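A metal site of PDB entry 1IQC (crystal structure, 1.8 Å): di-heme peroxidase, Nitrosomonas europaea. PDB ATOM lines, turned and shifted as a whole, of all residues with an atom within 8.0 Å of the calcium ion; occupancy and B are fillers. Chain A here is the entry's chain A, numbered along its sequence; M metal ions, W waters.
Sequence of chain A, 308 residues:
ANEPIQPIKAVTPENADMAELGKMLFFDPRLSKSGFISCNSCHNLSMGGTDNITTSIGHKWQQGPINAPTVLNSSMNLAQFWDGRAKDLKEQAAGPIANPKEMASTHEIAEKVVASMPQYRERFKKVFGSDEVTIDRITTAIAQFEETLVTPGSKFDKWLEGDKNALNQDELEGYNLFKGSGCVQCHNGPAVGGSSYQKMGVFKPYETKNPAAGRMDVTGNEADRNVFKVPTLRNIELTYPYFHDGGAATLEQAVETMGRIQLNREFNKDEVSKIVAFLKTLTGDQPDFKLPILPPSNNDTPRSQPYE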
ATOM      1  N   THR A  50      16.453  -3.812   3.506  1.00  0.00           N
ATOM      2  CA  THR A  50      17.052  -5.148   3.429  1.00  0.00           C
ATOM      3  C   THR A  50      18.043  -5.144   2.267  1.00  0.00           C
ATOM      4  O   THR A  50      18.275  -4.097   1.658  1.00  0.00           O
ATOM      5  CB  THR A  50      15.979  -6.264   3.197  1.00  0.00           C
ATOM      6  OG1 THR A  50      15.554  -6.266   1.832  1.00  0.00           O
ATOM      7  CG2 THR A  50      14.766  -6.047   4.087  1.00  0.00           C
ATOM      8  N   ASP A  51      18.643  -6.286   1.960  1.00  0.00           N
ATOM      9  CA  ASP A  51      19.588  -6.340   0.849  1.00  0.00           C
ATOM     10  C   ASP A  51      18.983  -7.009  -0.385  1.00  0.00           C
ATOM     11  O   ASP A  51      19.642  -7.148  -1.411  1.00  0.00           O
ATOM     12  CB  ASP A  51      20.880  -7.067   1.256  1.00  0.00           C
ATOM     13  CG  ASP A  51      20.618  -8.402   1.898  1.00  0.00           C
ATOM     14  OD1 ASP A  51      19.533  -8.966   1.673  1.00  0.00           O
ATOM     15  OD2 ASP A  51      21.508  -8.883   2.627  1.00  0.00           O
ATOM     16  N   ASN A  52      17.728  -7.412  -0.258  1.00  0.00           N
ATOM     17  CA  ASN A  52      16.980  -8.010  -1.360  1.00  0.00           C
ATOM     18  C   ASN A  52      17.644  -9.174  -2.076  1.00  0.00           C
ATOM     19  O   ASN A  52      17.549  -9.284  -3.301  1.00  0.00           O
ATOM     20  CB  ASN A  52      16.606  -6.905  -2.345  1.00  0.00           C
ATOM     21  CG  ASN A  52      15.670  -5.878  -1.723  1.00  0.00           C
ATOM     22  OD1 ASN A  52      14.495  -6.159  -1.457  1.00  0.00           O
ATOM     23  ND2 ASN A  52      16.192  -4.693  -1.481  1.00  0.00           N
ATOM     24  N   ILE A  53      18.327 -10.017  -1.320  1.00  0.00           N
ATOM     25  CA  ILE A  53      18.951 -11.219  -1.875  1.00  0.00           C
ATOM     26  C   ILE A  53      18.616 -12.373  -0.921  1.00  0.00           C
ATOM     27  O   ILE A  53      18.128 -12.131   0.186  1.00  0.00           O
ATOM     28  CB  ILE A  53      20.503 -11.068  -2.071  1.00  0.00           C
ATOM     29  CG1 ILE A  53      21.185 -10.518  -0.825  1.00  0.00           C
ATOM     30  CG2 ILE A  53      20.775 -10.197  -3.297  1.00  0.00           C
ATOM     31  CD1 ILE A  53      22.712 -10.442  -0.952  1.00  0.00           C
ATOM     32  N   THR A  54      18.832 -13.620  -1.345  1.00  0.00           N
ATOM     33  CA  THR A  54      18.472 -14.748  -0.484  1.00  0.00           C
ATOM     34  C   THR A  54      19.058 -14.692   0.921  1.00  0.00           C
ATOM     35  O   THR A  54      18.328 -14.856   1.894  1.00  0.00           O
ATOM     36  CB  THR A  54      18.827 -16.094  -1.162  1.00  0.00           C
ATOM     37  OG1 THR A  54      20.195 -16.094  -1.549  1.00  0.00           O
ATOM     38  CG2 THR A  54      17.936 -16.305  -2.373  1.00  0.00           C
ATOM     39  N   ASN A  67      18.066 -14.972   5.605  1.00  0.00           N
ATOM     40  CA  ASN A  67      17.609 -13.756   4.948  1.00  0.00           C
ATOM     41  C   ASN A  67      17.630 -12.561   5.910  1.00  0.00           C
ATOM     42  O   ASN A  67      17.165 -12.665   7.051  1.00  0.00           O
ATOM     43  CB  ASN A  67      16.194 -13.975   4.394  1.00  0.00           C
ATOM     44  CG  ASN A  67      15.755 -12.861   3.472  1.00  0.00           C
ATOM     45  OD1 ASN A  67      14.935 -12.030   3.846  1.00  0.00           O
ATOM     46  ND2 ASN A  67      16.305 -12.833   2.256  1.00  0.00           N
ATOM     47  N   ALA A  68      18.155 -11.430   5.454  1.00  0.00           N
ATOM     48  CA  ALA A  68      18.209 -10.240   6.289  1.00  0.00           C
ATOM     49  C   ALA A  68      16.845  -9.568   6.366  1.00  0.00           C
ATOM     50  O   ALA A  68      16.255  -9.210   5.337  1.00  0.00           O
ATOM     51  CB  ALA A  68      19.248  -9.258   5.735  1.00  0.00           C
ATOM     52  N   PRO A  69      16.304  -9.404   7.588  1.00  0.00           N
ATOM     53  CA  PRO A  69      15.005  -8.764   7.799  1.00  0.00           C
ATOM     54  C   PRO A  69      15.131  -7.259   7.659  1.00  0.00           C
ATOM     55  O   PRO A  69      16.233  -6.718   7.688  1.00  0.00           O
ATOM     56  CB  PRO A  69      14.644  -9.178   9.222  1.00  0.00           C
ATOM     57  CG  PRO A  69      16.003  -9.187   9.886  1.00  0.00           C
ATOM     58  CD  PRO A  69      16.861  -9.893   8.859  1.00  0.00           C
ATOM     59  N   THR A  70      14.005  -6.572   7.495  1.00  0.00           N
ATOM     60  CA  THR A  70      14.064  -5.129   7.344  1.00  0.00           C
ATOM     61  C   THR A  70      14.161  -4.404   8.668  1.00  0.00           C
ATOM     62  O   THR A  70      13.578  -4.827   9.675  1.00  0.00           O
ATOM     63  CB  THR A  70      12.823  -4.566   6.607  1.00  0.00           C
ATOM     64  OG1 THR A  70      12.954  -3.133   6.490  1.00  0.00           O
ATOM     65  CG2 THR A  70      11.559  -4.877   7.381  1.00  0.00           C
ATOM     66  N   TRP A  82      15.514 -13.482  13.827  1.00  0.00           N
ATOM     67  CA  TRP A  82      14.507 -14.494  13.526  1.00  0.00           C
ATOM     68  C   TRP A  82      14.168 -15.390  14.717  1.00  0.00           C
ATOM     69  O   TRP A  82      13.039 -15.863  14.827  1.00  0.00           O
ATOM     70  CB  TRP A  82      14.936 -15.363  12.347  1.00  0.00           C
ATOM     71  CG  TRP A  82      14.848 -14.694  10.986  1.00  0.00           C
ATOM     72  CD1 TRP A  82      15.847 -14.035  10.322  1.00  0.00           C
ATOM     73  CD2 TRP A  82      13.700 -14.660  10.127  1.00  0.00           C
ATOM     74  NE1 TRP A  82      15.388 -13.604   9.097  1.00  0.00           N
ATOM     75  CE2 TRP A  82      14.074 -13.969   8.958  1.00  0.00           C
ATOM     76  CE3 TRP A  82      12.389 -15.133  10.242  1.00  0.00           C
ATOM     77  CZ2 TRP A  82      13.186 -13.744   7.905  1.00  0.00           C
ATOM     78  CZ3 TRP A  82      11.508 -14.924   9.183  1.00  0.00           C
ATOM     79  CH2 TRP A  82      11.905 -14.237   8.031  1.00  0.00           C
ATOM     80  N   PRO A 231       7.447 -12.153  10.970  1.00  0.00           N
ATOM     81  CA  PRO A 231       7.931 -10.937  10.318  1.00  0.00           C
ATOM     82  C   PRO A 231       6.829  -9.903  10.114  1.00  0.00           C
ATOM     83  O   PRO A 231       5.653 -10.254   9.993  1.00  0.00           O
ATOM     84  CB  PRO A 231       8.454 -11.441   8.967  1.00  0.00           C
ATOM     85  CG  PRO A 231       8.779 -12.879   9.224  1.00  0.00           C
ATOM     86  CD  PRO A 231       7.635 -13.323  10.090  1.00  0.00           C
ATOM     87  N   ILE A 236       6.229  -5.131   2.868  1.00  0.00           N
ATOM     88  CA  ILE A 236       6.583  -6.457   2.357  1.00  0.00           C
ATOM     89  C   ILE A 236       6.851  -6.385   0.858  1.00  0.00           C
ATOM     90  O   ILE A 236       7.619  -7.179   0.316  1.00  0.00           O
ATOM     91  CB  ILE A 236       5.464  -7.482   2.668  1.00  0.00           C
ATOM     92  CG1 ILE A 236       5.975  -8.903   2.400  1.00  0.00           C
ATOM     93  CG2 ILE A 236       4.197  -7.165   1.879  1.00  0.00           C
ATOM     94  CD1 ILE A 236       7.101  -9.328   3.327  1.00  0.00           C
ATOM     95  N   LEU A 238       8.600  -4.336  -0.608  1.00  0.00           N
ATOM     96  CA  LEU A 238       9.994  -3.917  -0.838  1.00  0.00           C
ATOM     97  C   LEU A 238      11.071  -4.834  -0.294  1.00  0.00           C
ATOM     98  O   LEU A 238      12.254  -4.555  -0.479  1.00  0.00           O
ATOM     99  CB  LEU A 238      10.229  -2.546  -0.204  1.00  0.00           C
ATOM    100  CG  LEU A 238       9.131  -1.485  -0.303  1.00  0.00           C
ATOM    101  CD1 LEU A 238       9.627  -0.218   0.372  1.00  0.00           C
ATOM    102  CD2 LEU A 238       8.797  -1.215  -1.753  1.00  0.00           C
ATOM    103  N   THR A 239      10.684  -5.929   0.348  1.00  0.00           N
ATOM    104  CA  THR A 239      11.670  -6.789   0.979  1.00  0.00           C
ATOM    105  C   THR A 239      11.830  -8.220   0.479  1.00  0.00           C
ATOM    106  O   THR A 239      12.212  -9.111   1.240  1.00  0.00           O
ATOM    107  CB  THR A 239      11.407  -6.797   2.490  1.00  0.00           C
ATOM    108  OG1 THR A 239      10.138  -7.399   2.744  1.00  0.00           O
ATOM    109  CG2 THR A 239      11.384  -5.365   3.026  1.00  0.00           C
ATOM    110  N   TYR A 240      11.512  -8.439  -0.793  1.00  0.00           N
ATOM    111  CA  TYR A 240      11.691  -9.745  -1.449  1.00  0.00           C
ATOM    112  C   TYR A 240      13.201 -10.053  -1.397  1.00  0.00           C
ATOM    113  O   TYR A 240      14.021  -9.141  -1.288  1.00  0.00           O
ATOM    114  CB  TYR A 240      11.232  -9.620  -2.905  1.00  0.00           C
ATOM    115  CG  TYR A 240      11.741  -8.351  -3.552  1.00  0.00           C
ATOM    116  CD1 TYR A 240      13.035  -8.274  -4.078  1.00  0.00           C
ATOM    117  CD2 TYR A 240      10.996  -7.165  -3.476  1.00  0.00           C
ATOM    118  CE1 TYR A 240      13.572  -7.059  -4.500  1.00  0.00           C
ATOM    119  CE2 TYR A 240      11.525  -5.949  -3.892  1.00  0.00           C
ATOM    120  CZ  TYR A 240      12.814  -5.900  -4.401  1.00  0.00           C
ATOM    121  OH  TYR A 240      13.359  -4.687  -4.759  1.00  0.00           O
ATOM    122  N   PRO A 241      13.603 -11.351  -1.463  1.00  0.00           N
ATOM    123  CA  PRO A 241      12.754 -12.538  -1.556  1.00  0.00           C
ATOM    124  C   PRO A 241      12.157 -12.817  -0.179  1.00  0.00           C
ATOM    125  O   PRO A 241      12.573 -12.204   0.800  1.00  0.00           O
ATOM    126  CB  PRO A 241      13.726 -13.621  -2.029  1.00  0.00           C
ATOM    127  CG  PRO A 241      15.023 -13.198  -1.422  1.00  0.00           C
ATOM    128  CD  PRO A 241      15.016 -11.701  -1.678  1.00  0.00           C
ATOM    129  N   TYR A 242      11.218 -13.754  -0.105  1.00  0.00           N
ATOM    130  CA  TYR A 242      10.554 -14.015   1.174  1.00  0.00           C
ATOM    131  C   TYR A 242      10.907 -15.259   1.968  1.00  0.00           C
ATOM    132  O   TYR A 242      11.492 -16.204   1.442  1.00  0.00           O
ATOM    133  CB  TYR A 242       9.045 -13.900   0.955  1.00  0.00           C
ATOM    134  CG  TYR A 242       8.710 -12.609   0.264  1.00  0.00           C
ATOM    135  CD1 TYR A 242       8.457 -12.566  -1.111  1.00  0.00           C
ATOM    136  CD2 TYR A 242       8.727 -11.398   0.972  1.00  0.00           C
ATOM    137  CE1 TYR A 242       8.241 -11.344  -1.761  1.00  0.00           C
ATOM    138  CE2 TYR A 242       8.513 -10.183   0.328  1.00  0.00           C
ATOM    139  CZ  TYR A 242       8.269 -10.163  -1.030  1.00  0.00           C
ATOM    140  OH  TYR A 242       8.079  -8.952  -1.656  1.00  0.00           O
ATOM    141  N   PHE A 243      10.519 -15.233   3.243  1.00  0.00           N
ATOM    142  CA  PHE A 243      10.765 -16.282   4.228  1.00  0.00           C
ATOM    143  C   PHE A 243      12.224 -16.234   4.673  1.00  0.00           C
ATOM    144  O   PHE A 243      13.059 -15.622   4.014  1.00  0.00           O
ATOM    145  CB  PHE A 243      10.369 -17.650   3.663  1.00  0.00           C
ATOM    146  CG  PHE A 243       8.898 -17.769   3.374  1.00  0.00           C
ATOM    147  CD1 PHE A 243       8.434 -18.510   2.302  1.00  0.00           C
ATOM    148  CD2 PHE A 243       7.967 -17.087   4.163  1.00  0.00           C
ATOM    149  CE1 PHE A 243       7.069 -18.588   2.013  1.00  0.00           C
ATOM    150  CE2 PHE A 243       6.604 -17.151   3.892  1.00  0.00           C
ATOM    151  CZ  PHE A 243       6.154 -17.908   2.809  1.00  0.00           C
ATOM    152  N   HIS A 244      12.520 -16.869   5.798  1.00  0.00           N
ATOM    153  CA  HIS A 244      13.870 -16.833   6.352  1.00  0.00           C
ATOM    154  C   HIS A 244      14.971 -17.405   5.465  1.00  0.00           C
ATOM    155  O   HIS A 244      16.140 -17.075   5.649  1.00  0.00           O
ATOM    156  CB  HIS A 244      13.912 -17.502   7.718  1.00  0.00           C
ATOM    157  CG  HIS A 244      13.851 -18.994   7.668  1.00  0.00           C
ATOM    158  ND1 HIS A 244      12.664 -19.686   7.621  1.00  0.00           N
ATOM    159  CD2 HIS A 244      14.829 -19.923   7.640  1.00  0.00           C
ATOM    160  CE1 HIS A 244      12.905 -20.982   7.554  1.00  0.00           C
ATOM    161  NE2 HIS A 244      14.220 -21.160   7.565  1.00  0.00           N
ATOM    162  N   ASP A 245      14.629 -18.265   4.520  1.00  0.00           N
ATOM    163  CA  ASP A 245      15.652 -18.833   3.645  1.00  0.00           C
ATOM    164  C   ASP A 245      15.666 -18.093   2.308  1.00  0.00           C
ATOM    165  O   ASP A 245      16.465 -18.398   1.426  1.00  0.00           O
ATOM    166  CB  ASP A 245      15.421 -20.334   3.444  1.00  0.00           C
ATOM    167  CG  ASP A 245      14.130 -20.636   2.681  1.00  0.00           C
ATOM    168  OD1 ASP A 245      13.158 -19.859   2.784  1.00  0.00           O
ATOM    169  OD2 ASP A 245      14.094 -21.680   1.997  1.00  0.00           O
ATOM    170  N   GLY A 246      14.775 -17.113   2.168  1.00  0.00           N
ATOM    171  CA  GLY A 246      14.683 -16.359   0.940  1.00  0.00           C
ATOM    172  C   GLY A 246      14.201 -17.247  -0.196  1.00  0.00           C
ATOM    173  O   GLY A 246      14.418 -16.933  -1.366  1.00  0.00           O
ATOM    174  N   GLY A 247      13.526 -18.340   0.145  1.00  0.00           N
ATOM    175  CA  GLY A 247      13.059 -19.288  -0.852  1.00  0.00           C
ATOM    176  C   GLY A 247      11.884 -18.914  -1.751  1.00  0.00           C
ATOM    177  O   GLY A 247      11.737 -19.474  -2.833  1.00  0.00           O
ATOM    178  N   ALA A 248      11.036 -17.992  -1.295  1.00  0.00           N
ATOM    179  CA  ALA A 248       9.890 -17.558  -2.095  1.00  0.00           C
ATOM    180  C   ALA A 248      10.256 -16.231  -2.766  1.00  0.00           C
ATOM    181  O   ALA A 248      10.352 -15.204  -2.116  1.00  0.00           O
ATOM    182  CB  ALA A 248       8.666 -17.389  -1.210  1.00  0.00           C
HETATM  183 CA    CA M   1      13.025 -10.820   2.762  1.00  0.00          CA
HETATM  184  O   HOH W   1      10.740  -9.939   3.501  1.00  0.00           O
HETATM  185  O   HOH W   2      12.179 -12.713   4.128  1.00  0.00           O
HETATM  186  O   HOH W   3      14.984 -10.104   1.300  1.00  0.00           O
HETATM  187  O   HOH W   4      13.729  -9.267   4.577  1.00  0.00           O
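The calcium ion is bound by O of Thr 239 (2.4 Å), O of Pro 241 (2.4 Å), water W2 (2.5 Å), water W4 (2.5 Å), OD1 of Asn 67 (2.5 Å), water W3 (2.5 Å) and water W1 (2.6 Å).
The calcium ion has seven donor atoms within binding distance.
Water W3 lies within hydrogen-bond range of the backbone carbonyl oxygen (O) of Tyr 240 (2.9 Å) and the side-chain amide nitrogen (ND2) of Asn 67 (3.2 Å).
O of Ile 53 lies within hydrogen-bond range of ND2 of Asn 67 (2.8 Å).
The backbone carbonyl oxygen of Asn 67 is in hydrogen-bond range of the indole nitrogen of Trp 82.
ND2 of Asn 67 lies within hydrogen-bond range of O of Thr 54, 2.9 Å away.
N of Asn 67 lies within hydrogen-bond range of O of His 244, 2.9 Å away.
Within 4 Å of the calcium ion: Asn 67, Thr 239 and Pro 241.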
